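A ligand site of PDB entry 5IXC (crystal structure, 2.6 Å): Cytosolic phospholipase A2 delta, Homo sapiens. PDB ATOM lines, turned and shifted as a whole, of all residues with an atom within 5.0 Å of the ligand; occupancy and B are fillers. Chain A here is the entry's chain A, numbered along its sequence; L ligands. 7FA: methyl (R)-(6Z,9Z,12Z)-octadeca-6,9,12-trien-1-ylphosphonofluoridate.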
ATOM      1  N   GLY A 333       1.956  32.898 -38.038  1.00  0.00           N
ATOM      2  CA  GLY A 333       2.140  32.974 -36.592  1.00  0.00           C
ATOM      3  C   GLY A 333       2.983  34.151 -36.201  1.00  0.00           C
ATOM      4  O   GLY A 333       3.227  35.054 -36.998  1.00  0.00           O
ATOM      5  N   GLY A 334       3.447  34.136 -34.952  1.00  0.00           N
ATOM      6  CA  GLY A 334       4.217  35.246 -34.357  1.00  0.00           C
ATOM      7  C   GLY A 334       3.751  35.702 -32.982  1.00  0.00           C
ATOM      8  O   GLY A 334       3.920  36.868 -32.609  1.00  0.00           O
ATOM      9  N   GLY A 335       3.150  34.799 -32.209  1.00  0.00           N
ATOM     10  CA  GLY A 335       2.715  35.102 -30.846  1.00  0.00           C
ATOM     11  C   GLY A 335       1.877  36.353 -30.690  1.00  0.00           C
ATOM     12  O   GLY A 335       0.916  36.563 -31.440  1.00  0.00           O
ATOM     13  N   SER A 365      -1.049  29.718 -35.197  1.00  0.00           N
ATOM     14  CA  SER A 365      -0.444  30.110 -33.913  1.00  0.00           C
ATOM     15  C   SER A 365      -0.989  31.427 -33.301  1.00  0.00           C
ATOM     16  O   SER A 365      -2.176  31.501 -32.969  1.00  0.00           O
ATOM     17  CB  SER A 365       1.092  30.114 -34.022  1.00  0.00           C
ATOM     18  OG  SER A 365       1.631  30.041 -32.704  1.00  0.00           O
ATOM     19  N   GLY A 366      -0.157  32.450 -33.133  1.00  0.00           N
ATOM     20  CA  GLY A 366      -0.606  33.705 -32.526  1.00  0.00           C
ATOM     21  C   GLY A 366      -1.838  34.332 -33.170  1.00  0.00           C
ATOM     22  O   GLY A 366      -2.670  34.924 -32.474  1.00  0.00           O
ATOM     23  N   TRP A 369      -5.220  33.384 -31.762  1.00  0.00           N
ATOM     24  CA  TRP A 369      -5.612  34.029 -30.517  1.00  0.00           C
ATOM     25  C   TRP A 369      -6.595  35.163 -30.807  1.00  0.00           C
ATOM     26  O   TRP A 369      -7.650  35.266 -30.183  1.00  0.00           O
ATOM     27  CB  TRP A 369      -4.408  34.583 -29.774  1.00  0.00           C
ATOM     28  CG  TRP A 369      -3.372  33.549 -29.459  1.00  0.00           C
ATOM     29  CD1 TRP A 369      -3.480  32.187 -29.610  1.00  0.00           C
ATOM     30  CD2 TRP A 369      -2.071  33.780 -28.901  1.00  0.00           C
ATOM     31  NE1 TRP A 369      -2.335  31.582 -29.200  1.00  0.00           N
ATOM     32  CE2 TRP A 369      -1.456  32.533 -28.753  1.00  0.00           C
ATOM     33  CE3 TRP A 369      -1.381  34.929 -28.524  1.00  0.00           C
ATOM     34  CZ2 TRP A 369      -0.173  32.404 -28.230  1.00  0.00           C
ATOM     35  CZ3 TRP A 369      -0.112  34.802 -28.020  1.00  0.00           C
ATOM     36  CH2 TRP A 369       0.484  33.546 -27.879  1.00  0.00           C
ATOM     37  N   PHE A 404       1.925  32.789 -12.589  1.00  0.00           N
ATOM     38  CA  PHE A 404       2.789  31.786 -11.928  1.00  0.00           C
ATOM     39  C   PHE A 404       2.793  31.831 -10.399  1.00  0.00           C
ATOM     40  O   PHE A 404       3.730  31.342  -9.752  1.00  0.00           O
ATOM     41  CB  PHE A 404       4.216  31.922 -12.446  1.00  0.00           C
ATOM     42  CG  PHE A 404       4.347  31.648 -13.906  1.00  0.00           C
ATOM     43  CD1 PHE A 404       4.437  30.347 -14.372  1.00  0.00           C
ATOM     44  CD2 PHE A 404       4.330  32.689 -14.825  1.00  0.00           C
ATOM     45  CE1 PHE A 404       4.538  30.081 -15.728  1.00  0.00           C
ATOM     46  CE2 PHE A 404       4.428  32.435 -16.172  1.00  0.00           C
ATOM     47  CZ  PHE A 404       4.541  31.133 -16.631  1.00  0.00           C
ATOM     48  N   PHE A 428       2.123  18.410 -21.207  1.00  0.00           N
ATOM     49  CA  PHE A 428       2.498  19.812 -21.044  1.00  0.00           C
ATOM     50  C   PHE A 428       1.536  20.750 -21.796  1.00  0.00           C
ATOM     51  O   PHE A 428       1.208  21.822 -21.313  1.00  0.00           O
ATOM     52  CB  PHE A 428       3.913  20.041 -21.561  1.00  0.00           C
ATOM     53  CG  PHE A 428       4.609  21.246 -20.950  1.00  0.00           C
ATOM     54  CD1 PHE A 428       5.979  21.330 -20.981  1.00  0.00           C
ATOM     55  CD2 PHE A 428       3.910  22.295 -20.351  1.00  0.00           C
ATOM     56  CE1 PHE A 428       6.644  22.415 -20.424  1.00  0.00           C
ATOM     57  CE2 PHE A 428       4.562  23.384 -19.804  1.00  0.00           C
ATOM     58  CZ  PHE A 428       5.938  23.448 -19.842  1.00  0.00           C
ATOM     59  N   TRP A 432       0.041  24.292 -20.695  1.00  0.00           N
ATOM     60  CA  TRP A 432       0.180  25.453 -21.580  1.00  0.00           C
ATOM     61  C   TRP A 432      -1.168  26.097 -21.891  1.00  0.00           C
ATOM     62  O   TRP A 432      -1.279  27.310 -21.978  1.00  0.00           O
ATOM     63  CB  TRP A 432       0.895  25.054 -22.873  1.00  0.00           C
ATOM     64  CG  TRP A 432       0.970  26.100 -23.954  1.00  0.00           C
ATOM     65  CD1 TRP A 432       0.660  25.926 -25.257  1.00  0.00           C
ATOM     66  CD2 TRP A 432       1.397  27.463 -23.817  1.00  0.00           C
ATOM     67  NE1 TRP A 432       0.869  27.094 -25.953  1.00  0.00           N
ATOM     68  CE2 TRP A 432       1.315  28.055 -25.086  1.00  0.00           C
ATOM     69  CE3 TRP A 432       1.833  28.242 -22.735  1.00  0.00           C
ATOM     70  CZ2 TRP A 432       1.656  29.382 -25.314  1.00  0.00           C
ATOM     71  CZ3 TRP A 432       2.165  29.566 -22.962  1.00  0.00           C
ATOM     72  CH2 TRP A 432       2.074  30.122 -24.233  1.00  0.00           C
ATOM     73  N   VAL A 435      -2.153  28.152 -18.665  1.00  0.00           N
ATOM     74  CA  VAL A 435      -1.373  29.385 -18.487  1.00  0.00           C
ATOM     75  C   VAL A 435      -1.746  30.387 -19.585  1.00  0.00           C
ATOM     76  O   VAL A 435      -1.933  31.570 -19.321  1.00  0.00           O
ATOM     77  CB  VAL A 435       0.171  29.209 -18.404  1.00  0.00           C
ATOM     78  CG1 VAL A 435       0.546  27.924 -17.666  1.00  0.00           C
ATOM     79  CG2 VAL A 435       0.822  29.261 -19.768  1.00  0.00           C
ATOM     80  N   MET A 439      -3.000  34.111 -19.291  1.00  0.00           N
ATOM     81  CA  MET A 439      -2.275  35.258 -19.879  1.00  0.00           C
ATOM     82  C   MET A 439      -3.156  36.112 -20.784  1.00  0.00           C
ATOM     83  O   MET A 439      -2.969  37.312 -20.912  1.00  0.00           O
ATOM     84  CB  MET A 439      -1.046  34.782 -20.652  1.00  0.00           C
ATOM     85  CG  MET A 439       0.004  34.142 -19.765  1.00  0.00           C
ATOM     86  SD  MET A 439       1.444  33.611 -20.686  1.00  0.00           S
ATOM     87  CE  MET A 439       2.317  35.152 -20.796  1.00  0.00           C
ATOM     88  N   SER A 532      -0.886  26.864 -30.804  1.00  0.00           N
ATOM     89  CA  SER A 532       0.258  27.725 -30.513  1.00  0.00           C
ATOM     90  C   SER A 532       1.310  27.020 -29.684  1.00  0.00           C
ATOM     91  O   SER A 532       2.144  27.664 -29.046  1.00  0.00           O
ATOM     92  CB  SER A 532      -0.178  28.996 -29.787  1.00  0.00           C
ATOM     93  OG  SER A 532      -1.522  28.917 -29.431  1.00  0.00           O
ATOM     94  N   ASN A 533       1.294  25.695 -29.707  1.00  0.00           N
ATOM     95  CA  ASN A 533       2.217  24.966 -28.863  1.00  0.00           C
ATOM     96  C   ASN A 533       3.638  25.317 -29.202  1.00  0.00           C
ATOM     97  O   ASN A 533       4.021  25.402 -30.357  1.00  0.00           O
ATOM     98  CB  ASN A 533       2.009  23.472 -28.989  1.00  0.00           C
ATOM     99  CG  ASN A 533       3.065  22.686 -28.256  1.00  0.00           C
ATOM    100  OD1 ASN A 533       3.450  23.051 -27.133  1.00  0.00           O
ATOM    101  ND2 ASN A 533       3.544  21.616 -28.864  1.00  0.00           N
ATOM    102  N   ILE A 534       4.422  25.495 -28.152  1.00  0.00           N
ATOM    103  CA  ILE A 534       5.769  26.002 -28.262  1.00  0.00           C
ATOM    104  C   ILE A 534       6.753  25.037 -27.639  1.00  0.00           C
ATOM    105  O   ILE A 534       7.969  25.225 -27.732  1.00  0.00           O
ATOM    106  CB  ILE A 534       5.773  27.397 -27.597  1.00  0.00           C
ATOM    107  CG1 ILE A 534       5.440  28.456 -28.649  1.00  0.00           C
ATOM    108  CG2 ILE A 534       7.053  27.762 -26.861  1.00  0.00           C
ATOM    109  CD1 ILE A 534       6.203  28.347 -29.936  1.00  0.00           C
ATOM    110  N   PHE A 535       6.228  23.953 -27.069  1.00  0.00           N
ATOM    111  CA  PHE A 535       6.992  23.167 -26.140  1.00  0.00           C
ATOM    112  C   PHE A 535       7.378  21.798 -26.646  1.00  0.00           C
ATOM    113  O   PHE A 535       6.632  21.140 -27.370  1.00  0.00           O
ATOM    114  CB  PHE A 535       6.256  23.031 -24.823  1.00  0.00           C
ATOM    115  CG  PHE A 535       6.142  24.325 -24.107  1.00  0.00           C
ATOM    116  CD1 PHE A 535       7.272  24.928 -23.595  1.00  0.00           C
ATOM    117  CD2 PHE A 535       4.923  24.946 -23.981  1.00  0.00           C
ATOM    118  CE1 PHE A 535       7.190  26.136 -22.944  1.00  0.00           C
ATOM    119  CE2 PHE A 535       4.831  26.151 -23.330  1.00  0.00           C
ATOM    120  CZ  PHE A 535       5.965  26.747 -22.806  1.00  0.00           C
ATOM    121  N   LEU A 539      10.172  17.481 -22.040  1.00  0.00           N
ATOM    122  CA  LEU A 539      10.798  18.462 -21.140  1.00  0.00           C
ATOM    123  C   LEU A 539      11.795  17.779 -20.199  1.00  0.00           C
ATOM    124  O   LEU A 539      12.887  18.321 -19.937  1.00  0.00           O
ATOM    125  CB  LEU A 539       9.742  19.166 -20.316  1.00  0.00           C
ATOM    126  CG  LEU A 539       8.920  20.189 -21.077  1.00  0.00           C
ATOM    127  CD1 LEU A 539       9.623  21.535 -21.071  1.00  0.00           C
ATOM    128  CD2 LEU A 539       8.611  19.773 -22.513  1.00  0.00           C
ATOM    129  N   TRP A 582      12.263  34.267 -17.960  1.00  0.00           N
ATOM    130  CA  TRP A 582      11.447  33.031 -17.960  1.00  0.00           C
ATOM    131  C   TRP A 582      12.274  31.757 -17.751  1.00  0.00           C
ATOM    132  O   TRP A 582      11.968  30.693 -18.289  1.00  0.00           O
ATOM    133  CB  TRP A 582      10.470  32.915 -19.152  1.00  0.00           C
ATOM    134  CG  TRP A 582      11.040  32.975 -20.542  1.00  0.00           C
ATOM    135  CD1 TRP A 582      11.613  34.061 -21.147  1.00  0.00           C
ATOM    136  CD2 TRP A 582      11.011  31.935 -21.527  1.00  0.00           C
ATOM    137  NE1 TRP A 582      11.978  33.746 -22.431  1.00  0.00           N
ATOM    138  CE2 TRP A 582      11.614  32.449 -22.699  1.00  0.00           C
ATOM    139  CE3 TRP A 582      10.559  30.610 -21.527  1.00  0.00           C
ATOM    140  CZ2 TRP A 582      11.771  31.688 -23.851  1.00  0.00           C
ATOM    141  CZ3 TRP A 582      10.716  29.847 -22.688  1.00  0.00           C
ATOM    142  CH2 TRP A 582      11.310  30.396 -23.836  1.00  0.00           C
ATOM    143  N   PRO A 585      10.133  31.262 -13.695  1.00  0.00           N
ATOM    144  CA  PRO A 585       8.821  30.607 -13.700  1.00  0.00           C
ATOM    145  C   PRO A 585       8.888  29.110 -14.000  1.00  0.00           C
ATOM    146  O   PRO A 585       7.948  28.382 -13.700  1.00  0.00           O
ATOM    147  CB  PRO A 585       8.061  31.324 -14.831  1.00  0.00           C
ATOM    148  CG  PRO A 585       8.744  32.635 -14.969  1.00  0.00           C
ATOM    149  CD  PRO A 585      10.179  32.386 -14.647  1.00  0.00           C
ATOM    150  N   GLY A 586       9.986  28.678 -14.618  1.00  0.00           N
ATOM    151  CA  GLY A 586      10.256  27.271 -14.851  1.00  0.00           C
ATOM    152  C   GLY A 586      10.419  26.463 -13.562  1.00  0.00           C
ATOM    153  O   GLY A 586       9.899  25.352 -13.438  1.00  0.00           O
ATOM    154  N   LEU A 589       7.073  26.487 -11.555  1.00  0.00           N
ATOM    155  CA  LEU A 589       6.140  25.512 -12.136  1.00  0.00           C
ATOM    156  C   LEU A 589       6.536  24.085 -11.799  1.00  0.00           C
ATOM    157  O   LEU A 589       5.718  23.307 -11.313  1.00  0.00           O
ATOM    158  CB  LEU A 589       6.021  25.641 -13.662  1.00  0.00           C
ATOM    159  CG  LEU A 589       5.054  26.696 -14.244  1.00  0.00           C
ATOM    160  CD1 LEU A 589       4.909  26.463 -15.731  1.00  0.00           C
ATOM    161  CD2 LEU A 589       3.681  26.650 -13.584  1.00  0.00           C
ATOM    162  N   LEU A 647      14.013  22.293 -24.597  1.00  0.00           N
ATOM    163  CA  LEU A 647      12.867  22.847 -23.869  1.00  0.00           C
ATOM    164  C   LEU A 647      11.703  23.218 -24.802  1.00  0.00           C
ATOM    165  O   LEU A 647      10.528  22.979 -24.485  1.00  0.00           O
ATOM    166  CB  LEU A 647      13.312  24.074 -23.089  1.00  0.00           C
ATOM    167  CG  LEU A 647      12.591  24.377 -21.775  1.00  0.00           C
ATOM    168  CD1 LEU A 647      13.534  25.120 -20.827  1.00  0.00           C
ATOM    169  CD2 LEU A 647      11.325  25.185 -22.014  1.00  0.00           C
ATOM    170  N   TYR A 654       7.496  24.944 -37.635  1.00  0.00           N
ATOM    171  CA  TYR A 654       6.610  25.454 -36.568  1.00  0.00           C
ATOM    172  C   TYR A 654       6.516  26.965 -36.484  1.00  0.00           C
ATOM    173  O   TYR A 654       5.511  27.477 -35.983  1.00  0.00           O
ATOM    174  CB  TYR A 654       7.017  24.929 -35.195  1.00  0.00           C
ATOM    175  CG  TYR A 654       6.817  23.447 -35.037  1.00  0.00           C
ATOM    176  CD1 TYR A 654       7.886  22.601 -34.774  1.00  0.00           C
ATOM    177  CD2 TYR A 654       5.550  22.886 -35.157  1.00  0.00           C
ATOM    178  CE1 TYR A 654       7.706  21.231 -34.641  1.00  0.00           C
ATOM    179  CE2 TYR A 654       5.357  21.519 -35.034  1.00  0.00           C
ATOM    180  CZ  TYR A 654       6.441  20.689 -34.776  1.00  0.00           C
ATOM    181  OH  TYR A 654       6.279  19.324 -34.656  1.00  0.00           O
ATOM    182  N   PHE A 655       7.516  27.680 -36.981  1.00  0.00           N
ATOM    183  CA  PHE A 655       7.526  29.149 -36.876  1.00  0.00           C
ATOM    184  C   PHE A 655       7.506  29.945 -38.173  1.00  0.00           C
ATOM    185  O   PHE A 655       7.435  31.166 -38.121  1.00  0.00           O
ATOM    186  CB  PHE A 655       8.760  29.618 -36.128  1.00  0.00           C
ATOM    187  CG  PHE A 655       9.125  28.751 -34.986  1.00  0.00           C
ATOM    188  CD1 PHE A 655      10.089  27.775 -35.149  1.00  0.00           C
ATOM    189  CD2 PHE A 655       8.537  28.918 -33.746  1.00  0.00           C
ATOM    190  CE1 PHE A 655      10.451  26.968 -34.092  1.00  0.00           C
ATOM    191  CE2 PHE A 655       8.899  28.111 -32.688  1.00  0.00           C
ATOM    192  CZ  PHE A 655       9.863  27.133 -32.861  1.00  0.00           C
ATOM    193  N   LEU A 772       9.202  37.313 -30.200  1.00  0.00           N
ATOM    194  CA  LEU A 772       8.270  36.169 -30.109  1.00  0.00           C
ATOM    195  C   LEU A 772       8.007  35.729 -28.651  1.00  0.00           C
ATOM    196  O   LEU A 772       6.898  35.278 -28.325  1.00  0.00           O
ATOM    197  CB  LEU A 772       8.785  35.013 -30.967  1.00  0.00           C
ATOM    198  CG  LEU A 772       7.964  33.744 -31.074  1.00  0.00           C
ATOM    199  CD1 LEU A 772       6.549  33.994 -31.613  1.00  0.00           C
ATOM    200  CD2 LEU A 772       8.699  32.729 -31.918  1.00  0.00           C
ATOM    201  N   SER A 773       9.029  35.843 -27.800  1.00  0.00           N
ATOM    202  CA  SER A 773       8.946  35.489 -26.364  1.00  0.00           C
ATOM    203  C   SER A 773       8.004  36.373 -25.568  1.00  0.00           C
ATOM    204  O   SER A 773       7.399  35.929 -24.596  1.00  0.00           O
ATOM    205  CB  SER A 773      10.312  35.616 -25.687  1.00  0.00           C
ATOM    206  OG  SER A 773      11.176  34.564 -26.051  1.00  0.00           O
ATOM    207  N   MET A 775       5.269  38.444 -23.862  1.00  0.00           N
ATOM    208  CA  MET A 775       3.827  38.363 -23.661  1.00  0.00           C
ATOM    209  C   MET A 775       3.283  39.489 -22.794  1.00  0.00           C
ATOM    210  O   MET A 775       2.135  39.433 -22.365  1.00  0.00           O
ATOM    211  CB  MET A 775       3.452  37.013 -23.077  1.00  0.00           C
ATOM    212  CG  MET A 775       3.601  35.867 -24.063  1.00  0.00           C
ATOM    213  SD  MET A 775       2.100  35.338 -24.932  1.00  0.00           S
ATOM    214  CE  MET A 775       1.027  36.782 -24.891  1.00  0.00           C
HETATM  215  C1  7FA L   1       2.943  30.920 -30.430  1.00  0.00           C
HETATM  216  P1  7FA L   1       2.996  30.748 -32.233  1.00  0.00           P
HETATM  217  C2  7FA L   1       4.106  31.749 -29.877  1.00  0.00           C
HETATM  218  O2  7FA L   1       4.088  29.653 -32.606  1.00  0.00           O
HETATM  219  C3  7FA L   1       4.030  31.619 -28.366  1.00  0.00           C
HETATM  220  C4  7FA L   1       5.066  32.421 -27.582  1.00  0.00           C
HETATM  221  C5  7FA L   1       4.623  32.335 -26.124  1.00  0.00           C
HETATM  222  C6  7FA L   1       5.621  32.812 -25.083  1.00  0.00           C
HETATM  223  C7  7FA L   1       5.558  32.203 -23.892  1.00  0.00           C
HETATM  224  C8  7FA L   1       6.461  32.546 -22.732  1.00  0.00           C
HETATM  225  C9  7FA L   1       5.863  31.892 -21.500  1.00  0.00           C
HETATM  226  CM  7FA L   1       5.151  29.961 -33.492  1.00  0.00           C
HETATM  227  C10 7FA L   1       6.141  30.629 -21.210  1.00  0.00           C
HETATM  228  C11 7FA L   1       5.509  29.968 -20.005  1.00  0.00           C
HETATM  229  C12 7FA L   1       6.473  29.085 -19.254  1.00  0.00           C
HETATM  230  C13 7FA L   1       6.245  27.778 -19.151  1.00  0.00           C
HETATM  231  C14 7FA L   1       7.225  26.913 -18.396  1.00  0.00           C
HETATM  232  C15 7FA L   1       8.471  26.606 -19.226  1.00  0.00           C
HETATM  233  C16 7FA L   1       9.674  26.317 -18.345  1.00  0.00           C
HETATM  234  C17 7FA L   1       9.505  25.016 -17.561  1.00  0.00           C
HETATM  235  C18 7FA L   1      10.825  24.529 -16.995  1.00  0.00           C
HETATM  236  O1  7FA L   1       3.198  32.023 -32.932  1.00  0.00           O
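OG of Ser 365 is covalently linked to P1 of the ligand.
The backbone NH (N) of Gly 335 is in hydrogen-bond range of an oxygen (O1) of the ligand, at 2.9 Å.
N of Gly 334 sits at hydrogen-bond distance from O1 of the ligand, 2.9 Å away.
N of Gly 366 is in hydrogen-bond range of O1 of the ligand (3.4 Å).
O of Ser 532 is in hydrogen-bond range of NE1 of Trp 432 (3.4 Å).
OG of Ser 532 sits at hydrogen-bond distance from NE1 of Trp 369 (2.8 Å).
N of Phe 535 sits at hydrogen-bond distance from OD1 of Asn 533, at 2.9 Å.
Residues that only touch the ligand: Leu 772, Ile 534, Gly 586, Tyr 654, Phe 655, Leu 589, Ser 773, Ser 532, Phe 404, Met 775, Phe 535, Trp 432, Gly 333 and Phe 428.
Hydrophobic or aromatic side chains within 4 Å of the ligand: Phe 404, Phe 428, Trp 432, Ile 534, Phe 535, Leu 589, Phe 655, Leu 772 and Met 775.
Of the 26 residues printed, 18 come within 4 Å of the ligand.
The nearest printed residue that does not touch the ligand is Trp 369 (4.1 Å).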
